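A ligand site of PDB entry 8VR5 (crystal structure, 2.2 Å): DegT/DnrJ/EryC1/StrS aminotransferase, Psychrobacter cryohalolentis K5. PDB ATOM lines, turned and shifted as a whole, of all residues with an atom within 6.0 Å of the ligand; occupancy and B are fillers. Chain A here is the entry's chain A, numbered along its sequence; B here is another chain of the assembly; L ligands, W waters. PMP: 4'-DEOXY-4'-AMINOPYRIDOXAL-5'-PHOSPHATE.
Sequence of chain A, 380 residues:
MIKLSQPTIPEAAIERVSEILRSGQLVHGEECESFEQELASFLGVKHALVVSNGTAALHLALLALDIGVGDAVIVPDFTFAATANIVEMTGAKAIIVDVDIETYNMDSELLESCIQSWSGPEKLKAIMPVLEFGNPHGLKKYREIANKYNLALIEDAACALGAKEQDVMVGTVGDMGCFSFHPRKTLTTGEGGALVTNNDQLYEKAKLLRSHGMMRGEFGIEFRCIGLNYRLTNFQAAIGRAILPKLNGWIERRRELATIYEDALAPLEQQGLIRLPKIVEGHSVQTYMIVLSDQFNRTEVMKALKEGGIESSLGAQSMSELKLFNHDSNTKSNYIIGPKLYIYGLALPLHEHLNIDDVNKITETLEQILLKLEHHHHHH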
ATOM      1  N   ASN A  53      17.050 -12.063 -33.263  1.00  0.00           N
ATOM      2  CA  ASN A  53      16.350 -12.708 -32.158  1.00  0.00           C
ATOM      3  C   ASN A  53      17.322 -13.001 -31.027  1.00  0.00           C
ATOM      4  O   ASN A  53      18.500 -12.703 -31.127  1.00  0.00           O
ATOM      5  CB  ASN A  53      15.636 -13.963 -32.645  1.00  0.00           C
ATOM      6  CG  ASN A  53      16.564 -14.921 -33.364  1.00  0.00           C
ATOM      7  OD1 ASN A  53      17.422 -15.534 -32.754  1.00  0.00           O
ATOM      8  ND2 ASN A  53      16.363 -15.113 -34.658  1.00  0.00           N
ATOM      9  N   GLY A  54      16.841 -13.564 -29.921  1.00  0.00           N
ATOM     10  CA  GLY A  54      17.693 -13.795 -28.771  1.00  0.00           C
ATOM     11  C   GLY A  54      18.698 -14.929 -29.005  1.00  0.00           C
ATOM     12  O   GLY A  54      19.817 -14.892 -28.476  1.00  0.00           O
ATOM     13  N   THR A  55      18.292 -15.907 -29.819  1.00  0.00           N
ATOM     14  CA  THR A  55      19.178 -17.003 -30.168  1.00  0.00           C
ATOM     15  C   THR A  55      20.365 -16.480 -30.981  1.00  0.00           C
ATOM     16  O   THR A  55      21.496 -16.877 -30.776  1.00  0.00           O
ATOM     17  CB  THR A  55      18.390 -18.090 -30.907  1.00  0.00           C
ATOM     18  OG1 THR A  55      17.243 -18.450 -30.132  1.00  0.00           O
ATOM     19  CG2 THR A  55      19.271 -19.282 -31.251  1.00  0.00           C
ATOM     20  N   ALA A  56      20.109 -15.557 -31.908  1.00  0.00           N
ATOM     21  CA  ALA A  56      21.178 -14.951 -32.667  1.00  0.00           C
ATOM     22  C   ALA A  56      22.180 -14.215 -31.764  1.00  0.00           C
ATOM     23  O   ALA A  56      23.367 -14.182 -32.087  1.00  0.00           O
ATOM     24  CB  ALA A  56      20.620 -13.984 -33.686  1.00  0.00           C
ATOM     25  N   LEU A  58      23.025 -14.917 -28.623  1.00  0.00           N
ATOM     26  CA  LEU A  58      23.788 -16.005 -28.052  1.00  0.00           C
ATOM     27  C   LEU A  58      24.802 -16.541 -29.072  1.00  0.00           C
ATOM     28  O   LEU A  58      25.971 -16.721 -28.772  1.00  0.00           O
ATOM     29  CB  LEU A  58      22.837 -17.102 -27.547  1.00  0.00           C
ATOM     30  CG  LEU A  58      22.034 -16.720 -26.315  1.00  0.00           C
ATOM     31  CD1 LEU A  58      20.928 -17.696 -26.089  1.00  0.00           C
ATOM     32  CD2 LEU A  58      22.893 -16.676 -25.049  1.00  0.00           C
ATOM     33  N   THR A  79      15.934 -24.233 -18.667  1.00  0.00           N
ATOM     34  CA  THR A  79      15.958 -23.098 -19.581  1.00  0.00           C
ATOM     35  C   THR A  79      15.168 -23.485 -20.813  1.00  0.00           C
ATOM     36  O   THR A  79      14.610 -24.589 -20.870  1.00  0.00           O
ATOM     37  CB  THR A  79      17.381 -22.711 -19.944  1.00  0.00           C
ATOM     38  OG1 THR A  79      17.391 -21.505 -20.717  1.00  0.00           O
ATOM     39  CG2 THR A  79      18.090 -23.827 -20.690  1.00  0.00           C
ATOM     40  N   PHE A  80      15.067 -22.555 -21.761  1.00  0.00           N
ATOM     41  CA  PHE A  80      14.541 -22.889 -23.071  1.00  0.00           C
ATOM     42  C   PHE A  80      15.675 -23.543 -23.859  1.00  0.00           C
ATOM     43  O   PHE A  80      16.823 -23.224 -23.630  1.00  0.00           O
ATOM     44  CB  PHE A  80      13.967 -21.644 -23.782  1.00  0.00           C
ATOM     45  CG  PHE A  80      13.419 -21.890 -25.174  1.00  0.00           C
ATOM     46  CD1 PHE A  80      14.065 -21.382 -26.292  1.00  0.00           C
ATOM     47  CD2 PHE A  80      12.314 -22.702 -25.362  1.00  0.00           C
ATOM     48  CE1 PHE A  80      13.585 -21.633 -27.567  1.00  0.00           C
ATOM     49  CE2 PHE A  80      11.823 -22.950 -26.647  1.00  0.00           C
ATOM     50  CZ  PHE A  80      12.471 -22.426 -27.760  1.00  0.00           C
ATOM     51  N   ALA A  82      17.025 -23.324 -26.646  1.00  0.00           N
ATOM     52  CA  ALA A  82      17.942 -22.512 -27.420  1.00  0.00           C
ATOM     53  C   ALA A  82      19.297 -22.405 -26.715  1.00  0.00           C
ATOM     54  O   ALA A  82      20.340 -22.395 -27.365  1.00  0.00           O
ATOM     55  CB  ALA A  82      17.342 -21.154 -27.673  1.00  0.00           C
ATOM     56  N   THR A  83      19.296 -22.257 -25.385  1.00  0.00           N
ATOM     57  CA  THR A  83      20.519 -22.007 -24.622  1.00  0.00           C
ATOM     58  C   THR A  83      21.540 -23.112 -24.904  1.00  0.00           C
ATOM     59  O   THR A  83      22.668 -22.803 -25.281  1.00  0.00           O
ATOM     60  CB  THR A  83      20.266 -21.933 -23.110  1.00  0.00           C
ATOM     61  OG1 THR A  83      19.223 -21.002 -22.802  1.00  0.00           O
ATOM     62  CG2 THR A  83      21.520 -21.616 -22.336  1.00  0.00           C
ATOM     63  N   VAL A 130      21.612 -18.734 -17.206  1.00  0.00           N
ATOM     64  CA  VAL A 130      20.378 -18.075 -17.603  1.00  0.00           C
ATOM     65  C   VAL A 130      19.849 -17.282 -16.432  1.00  0.00           C
ATOM     66  O   VAL A 130      19.810 -17.782 -15.311  1.00  0.00           O
ATOM     67  CB  VAL A 130      19.357 -19.106 -18.116  1.00  0.00           C
ATOM     68  CG1 VAL A 130      17.975 -18.480 -18.352  1.00  0.00           C
ATOM     69  CG2 VAL A 130      19.871 -19.803 -19.396  1.00  0.00           C
ATOM     70  N   GLU A 132      16.849 -16.626 -15.311  1.00  0.00           N
ATOM     71  CA  GLU A 132      15.601 -17.198 -15.761  1.00  0.00           C
ATOM     72  C   GLU A 132      14.410 -16.416 -15.215  1.00  0.00           C
ATOM     73  O   GLU A 132      14.357 -16.036 -14.046  1.00  0.00           O
ATOM     74  CB  GLU A 132      15.556 -18.669 -15.352  1.00  0.00           C
ATOM     75  CG  GLU A 132      14.340 -19.447 -15.821  1.00  0.00           C
ATOM     76  CD  GLU A 132      14.192 -19.490 -17.327  1.00  0.00           C
ATOM     77  OE1 GLU A 132      14.222 -20.603 -17.874  1.00  0.00           O
ATOM     78  OE2 GLU A 132      14.014 -18.409 -17.927  1.00  0.00           O
ATOM     79  N   ASP A 156      22.887 -15.443 -20.629  1.00  0.00           N
ATOM     80  CA  ASP A 156      21.646 -15.606 -21.376  1.00  0.00           C
ATOM     81  C   ASP A 156      20.594 -14.872 -20.552  1.00  0.00           C
ATOM     82  O   ASP A 156      19.924 -15.424 -19.664  1.00  0.00           O
ATOM     83  CB  ASP A 156      21.327 -17.067 -21.702  1.00  0.00           C
ATOM     84  CG  ASP A 156      20.050 -17.201 -22.528  1.00  0.00           C
ATOM     85  OD1 ASP A 156      19.486 -16.170 -22.843  1.00  0.00           O
ATOM     86  OD2 ASP A 156      19.605 -18.362 -22.823  1.00  0.00           O
ATOM     87  N   ALA A 158      18.032 -13.601 -21.952  1.00  0.00           N
ATOM     88  CA  ALA A 158      16.895 -13.598 -22.854  1.00  0.00           C
ATOM     89  C   ALA A 158      15.701 -12.902 -22.209  1.00  0.00           C
ATOM     90  O   ALA A 158      15.029 -12.081 -22.858  1.00  0.00           O
ATOM     91  CB  ALA A 158      16.552 -15.003 -23.272  1.00  0.00           C
ATOM     92  N   CYS A 159      15.422 -13.270 -20.943  1.00  0.00           N
ATOM     93  CA  CYS A 159      14.198 -12.908 -20.254  1.00  0.00           C
ATOM     94  C   CYS A 159      14.371 -11.757 -19.268  1.00  0.00           C
ATOM     95  O   CYS A 159      13.475 -11.499 -18.471  1.00  0.00           O
ATOM     96  CB  CYS A 159      13.712 -14.019 -19.315  1.00  0.00           C
ATOM     97  SG  CYS A 159      13.415 -15.626 -20.087  1.00  0.00           S
ATOM     98  N   PHE A 179      19.907 -10.653 -24.908  1.00  0.00           N
ATOM     99  CA  PHE A 179      18.500 -10.394 -24.638  1.00  0.00           C
ATOM    100  C   PHE A 179      17.639 -10.871 -25.806  1.00  0.00           C
ATOM    101  O   PHE A 179      18.087 -10.831 -26.938  1.00  0.00           O
ATOM    102  CB  PHE A 179      18.283  -8.897 -24.404  1.00  0.00           C
ATOM    103  CG  PHE A 179      19.088  -8.305 -23.276  1.00  0.00           C
ATOM    104  CD1 PHE A 179      20.197  -7.526 -23.549  1.00  0.00           C
ATOM    105  CD2 PHE A 179      18.687  -8.473 -21.943  1.00  0.00           C
ATOM    106  CE1 PHE A 179      20.919  -6.944 -22.515  1.00  0.00           C
ATOM    107  CE2 PHE A 179      19.415  -7.885 -20.913  1.00  0.00           C
ATOM    108  CZ  PHE A 179      20.526  -7.119 -21.204  1.00  0.00           C
ATOM    109  N   SER A 180      16.416 -11.337 -25.488  1.00  0.00           N
ATOM    110  CA  SER A 180      15.389 -11.684 -26.453  1.00  0.00           C
ATOM    111  C   SER A 180      14.284 -10.648 -26.409  1.00  0.00           C
ATOM    112  O   SER A 180      13.873 -10.241 -25.322  1.00  0.00           O
ATOM    113  CB  SER A 180      14.816 -13.066 -26.160  1.00  0.00           C
ATOM    114  OG  SER A 180      13.686 -13.305 -26.984  1.00  0.00           O
ATOM    115  N   PHE A 181      13.736 -10.332 -27.594  1.00  0.00           N
ATOM    116  CA  PHE A 181      12.579  -9.461 -27.749  1.00  0.00           C
ATOM    117  C   PHE A 181      11.422 -10.259 -28.357  1.00  0.00           C
ATOM    118  O   PHE A 181      10.567  -9.740 -29.065  1.00  0.00           O
ATOM    119  CB  PHE A 181      12.883  -8.251 -28.655  1.00  0.00           C
ATOM    120  CG  PHE A 181      14.103  -7.430 -28.281  1.00  0.00           C
ATOM    121  CD1 PHE A 181      14.615  -7.445 -27.002  1.00  0.00           C
ATOM    122  CD2 PHE A 181      14.745  -6.658 -29.243  1.00  0.00           C
ATOM    123  CE1 PHE A 181      15.721  -6.682 -26.675  1.00  0.00           C
ATOM    124  CE2 PHE A 181      15.845  -5.885 -28.908  1.00  0.00           C
ATOM    125  CZ  PHE A 181      16.329  -5.887 -27.626  1.00  0.00           C
ATOM    126  N   HIS A 182      11.406 -11.554 -28.055  1.00  0.00           N
ATOM    127  CA  HIS A 182      10.344 -12.467 -28.415  1.00  0.00           C
ATOM    128  C   HIS A 182       9.026 -12.033 -27.772  1.00  0.00           C
ATOM    129  O   HIS A 182       9.001 -11.360 -26.742  1.00  0.00           O
ATOM    130  CB  HIS A 182      10.806 -13.862 -27.992  1.00  0.00           C
ATOM    131  CG  HIS A 182       9.835 -14.910 -28.313  1.00  0.00           C
ATOM    132  ND1 HIS A 182       8.749 -15.200 -27.503  1.00  0.00           N
ATOM    133  CD2 HIS A 182       9.781 -15.720 -29.369  1.00  0.00           C
ATOM    134  CE1 HIS A 182       8.062 -16.188 -28.075  1.00  0.00           C
ATOM    135  NE2 HIS A 182       8.679 -16.517 -29.212  1.00  0.00           N
ATOM    136  N   ARG A 184       6.877 -13.230 -25.905  1.00  0.00           N
ATOM    137  CA  ARG A 184       6.615 -13.630 -24.521  1.00  0.00           C
ATOM    138  C   ARG A 184       7.411 -12.758 -23.560  1.00  0.00           C
ATOM    139  O   ARG A 184       7.183 -12.863 -22.374  1.00  0.00           O
ATOM    140  CB  ARG A 184       6.964 -15.102 -24.226  1.00  0.00           C
ATOM    141  CG  ARG A 184       5.761 -16.043 -24.065  1.00  0.00           C
ATOM    142  CD  ARG A 184       5.481 -16.939 -25.284  1.00  0.00           C
ATOM    143  NE  ARG A 184       5.904 -18.342 -25.177  1.00  0.00           N
ATOM    144  CZ  ARG A 184       5.956 -19.211 -26.195  1.00  0.00           C
ATOM    145  NH1 ARG A 184       5.801 -18.803 -27.440  1.00  0.00           N
ATOM    146  NH2 ARG A 184       6.198 -20.492 -25.966  1.00  0.00           N
ATOM    147  N   LYS A 185       8.381 -11.971 -24.054  1.00  0.00           N
ATOM    148  CA  LYS A 185       9.231 -11.153 -23.197  1.00  0.00           C
ATOM    149  C   LYS A 185       8.538  -9.807 -23.025  1.00  0.00           C
ATOM    150  O   LYS A 185       7.511  -9.565 -23.617  1.00  0.00           O
ATOM    151  CB  LYS A 185      10.647 -11.034 -23.787  1.00  0.00           C
ATOM    152  CG  LYS A 185      11.365 -12.347 -24.088  1.00  0.00           C
ATOM    153  CD  LYS A 185      11.312 -13.394 -22.978  1.00  0.00           C
ATOM    154  CE  LYS A 185      12.102 -14.680 -23.198  1.00  0.00           C
ATOM    155  NZ  LYS A 185      12.063 -15.583 -22.003  1.00  0.00           N
ATOM    156  N   GLU A 191      10.091 -10.496 -33.363  1.00  0.00           N
ATOM    157  CA  GLU A 191      11.298 -11.259 -33.128  1.00  0.00           C
ATOM    158  C   GLU A 191      12.393 -10.221 -33.001  1.00  0.00           C
ATOM    159  O   GLU A 191      12.317  -9.178 -33.657  1.00  0.00           O
ATOM    160  CB  GLU A 191      11.658 -12.184 -34.305  1.00  0.00           C
ATOM    161  CG  GLU A 191      10.685 -13.349 -34.527  1.00  0.00           C
ATOM    162  CD  GLU A 191      10.896 -14.602 -33.696  1.00  0.00           C
ATOM    163  OE1 GLU A 191      11.817 -14.640 -32.834  1.00  0.00           O
ATOM    164  OE2 GLU A 191      10.179 -15.585 -33.965  1.00  0.00           O
ATOM    165  N   GLY A 192      13.375 -10.479 -32.138  1.00  0.00           N
ATOM    166  CA  GLY A 192      14.447  -9.523 -31.962  1.00  0.00           C
ATOM    167  C   GLY A 192      15.283  -9.857 -30.737  1.00  0.00           C
ATOM    168  O   GLY A 192      14.958 -10.771 -29.991  1.00  0.00           O
ATOM    169  N   GLY A 193      16.442  -9.218 -30.652  1.00  0.00           N
ATOM    170  CA  GLY A 193      17.350  -9.482 -29.570  1.00  0.00           C
ATOM    171  C   GLY A 193      18.470  -8.441 -29.571  1.00  0.00           C
ATOM    172  O   GLY A 193      18.507  -7.542 -30.412  1.00  0.00           O
ATOM    173  N   HIS B 212      14.470 -24.279 -33.371  1.00  0.00           N
ATOM    174  CA  HIS B 212      14.898 -24.955 -32.174  1.00  0.00           C
ATOM    175  C   HIS B 212      14.519 -26.428 -32.172  1.00  0.00           C
ATOM    176  O   HIS B 212      14.338 -27.020 -31.123  1.00  0.00           O
ATOM    177  CB  HIS B 212      14.255 -24.303 -30.964  1.00  0.00           C
ATOM    178  CG  HIS B 212      14.519 -22.837 -30.933  1.00  0.00           C
ATOM    179  ND1 HIS B 212      15.799 -22.331 -30.808  1.00  0.00           N
ATOM    180  CD2 HIS B 212      13.664 -21.770 -31.021  1.00  0.00           C
ATOM    181  CE1 HIS B 212      15.724 -20.995 -30.816  1.00  0.00           C
ATOM    182  NE2 HIS B 212      14.431 -20.621 -30.915  1.00  0.00           N
ATOM    183  N   ASN B 229      17.189 -20.144 -34.540  1.00  0.00           N
ATOM    184  CA  ASN B 229      15.997 -19.363 -34.774  1.00  0.00           C
ATOM    185  C   ASN B 229      16.187 -18.536 -36.035  1.00  0.00           C
ATOM    186  O   ASN B 229      17.005 -17.597 -36.050  1.00  0.00           O
ATOM    187  CB  ASN B 229      15.664 -18.482 -33.577  1.00  0.00           C
ATOM    188  CG  ASN B 229      14.384 -17.708 -33.785  1.00  0.00           C
ATOM    189  OD1 ASN B 229      13.749 -17.799 -34.838  1.00  0.00           O
ATOM    190  ND2 ASN B 229      13.999 -16.945 -32.761  1.00  0.00           N
ATOM    191  N   ARG B 231      13.212 -17.654 -37.764  1.00  0.00           N
ATOM    192  CA  ARG B 231      11.804 -17.396 -38.054  1.00  0.00           C
ATOM    193  C   ARG B 231      11.622 -15.976 -38.548  1.00  0.00           C
ATOM    194  O   ARG B 231      12.383 -15.042 -38.195  1.00  0.00           O
ATOM    195  CB  ARG B 231      10.901 -17.611 -36.847  1.00  0.00           C
ATOM    196  CG  ARG B 231      10.944 -19.035 -36.325  1.00  0.00           C
ATOM    197  CD  ARG B 231       9.859 -19.336 -35.313  1.00  0.00           C
ATOM    198  NE  ARG B 231      10.023 -18.398 -34.201  1.00  0.00           N
ATOM    199  CZ  ARG B 231      10.430 -18.701 -32.963  1.00  0.00           C
ATOM    200  NH1 ARG B 231      10.546 -19.961 -32.577  1.00  0.00           N
ATOM    201  NH2 ARG B 231      10.704 -17.721 -32.126  1.00  0.00           N
HETATM  202  N1  PMP L   1      17.132 -18.229 -23.799  1.00  0.00           N
HETATM  203  C2  PMP L   1      16.040 -18.242 -23.058  1.00  0.00           C
HETATM  204  C2A PMP L   1      16.237 -18.418 -21.593  1.00  0.00           C
HETATM  205  C3  PMP L   1      14.769 -18.018 -23.635  1.00  0.00           C
HETATM  206  O3  PMP L   1      13.631 -17.988 -22.843  1.00  0.00           O
HETATM  207  C4  PMP L   1      14.667 -17.833 -25.018  1.00  0.00           C
HETATM  208  C4A PMP L   1      13.344 -17.600 -25.705  1.00  0.00           C
HETATM  209  N4A PMP L   1      12.150 -17.690 -24.854  1.00  0.00           N
HETATM  210  C5  PMP L   1      15.840 -17.837 -25.785  1.00  0.00           C
HETATM  211  C6  PMP L   1      17.039 -18.061 -25.124  1.00  0.00           C
HETATM  212  C5A PMP L   1      15.828 -17.649 -27.270  1.00  0.00           C
HETATM  213  O4P PMP L   1      15.337 -16.328 -27.636  1.00  0.00           O
HETATM  214  P   PMP L   1      14.518 -16.045 -28.990  1.00  0.00           P
HETATM  215  O1P PMP L   1      14.436 -14.560 -29.107  1.00  0.00           O
HETATM  216  O2P PMP L   1      15.284 -16.673 -30.120  1.00  0.00           O
HETATM  217  O3P PMP L   1      13.186 -16.703 -28.759  1.00  0.00           O
HETATM  218  O   HOH W   1      13.158 -19.526 -20.396  1.00  0.00           O
HETATM  219  O   HOH W   2      12.580 -18.935 -29.942  1.00  0.00           O
HETATM  220  O   HOH W   3      12.923 -13.041 -30.907  1.00  0.00           O
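The side-chain hydroxyl of Ser 180 lies within hydrogen-bond range of an oxygen (O1P) of the ligand (2.6 Å). An oxygen (O2P) of the ligand lies within hydrogen-bond range of the backbone NH (N) of Thr 55, at 3.1 Å. O2P of the ligand lies within hydrogen-bond range of OG1 of Thr 55 (2.6 Å). A nitrogen (N1) of the ligand lies within hydrogen-bond range of the side-chain carboxylate of Asp 156 (2.7 Å). O1P of the ligand is in hydrogen-bond range of N of Gly 54 (2.7 Å). ND2 of Asn 229 of chain B lies within hydrogen-bond range of O2P of the ligand (2.9 Å). The side-chain amino group of Lys 185 lies within hydrogen-bond range of an oxygen (O3) of the ligand, 3.0 Å away. The side-chain sulfur (SG) of Cys 159 lies within hydrogen-bond range of an oxygen (O3) of the ligand, 3.6 Å away.
N of Ser 180 sits at hydrogen-bond distance from O of Ala 158 (3.1 Å). The side-chain hydroxyl of Ser 180 is in hydrogen-bond range of the backbone NH of His 182, 3.1 Å away. The side-chain carboxylate (OD1) of Asp 156 lies within hydrogen-bond range of the backbone NH (N) of Ala 158 (3.1 Å). The side-chain carboxylate of Asp 156 sits at hydrogen-bond distance from the side-chain hydroxyl of Thr 83. OD1 of Asn 53 is in hydrogen-bond range of N of Ala 56, 2.8 Å away. N of Arg 184 lies close to ND1 of His 182 (3.2 Å). OE2 of Glu 132 is in hydrogen-bond range of SG of Cys 159 (3.6 Å). O of Gly 192 lies within hydrogen-bond range of N of Phe 181, at 2.7 Å.
Residues that only touch the ligand: Asn 53, Thr 79, Phe 80, Ala 82, Thr 83, Val 130, Ala 158, His 182 and Gly 192. Hydrophobic or aromatic side chains within 4 Å of the ligand: Phe 80, Ala 82, Val 130, Ala 158 and His 182.
Water W2 lies within hydrogen-bond range of O3P of the ligand (2.6 Å), NE2 of His 212 of chain B (2.7 Å) and NH2 of Arg 231 of chain B (3.1 Å). Water W3 lies within hydrogen-bond range of OE1 of Glu 191, O1P of the ligand and N of Gly 192. Water W1 bridges OE2 of Glu 132 and O3 of the ligand.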
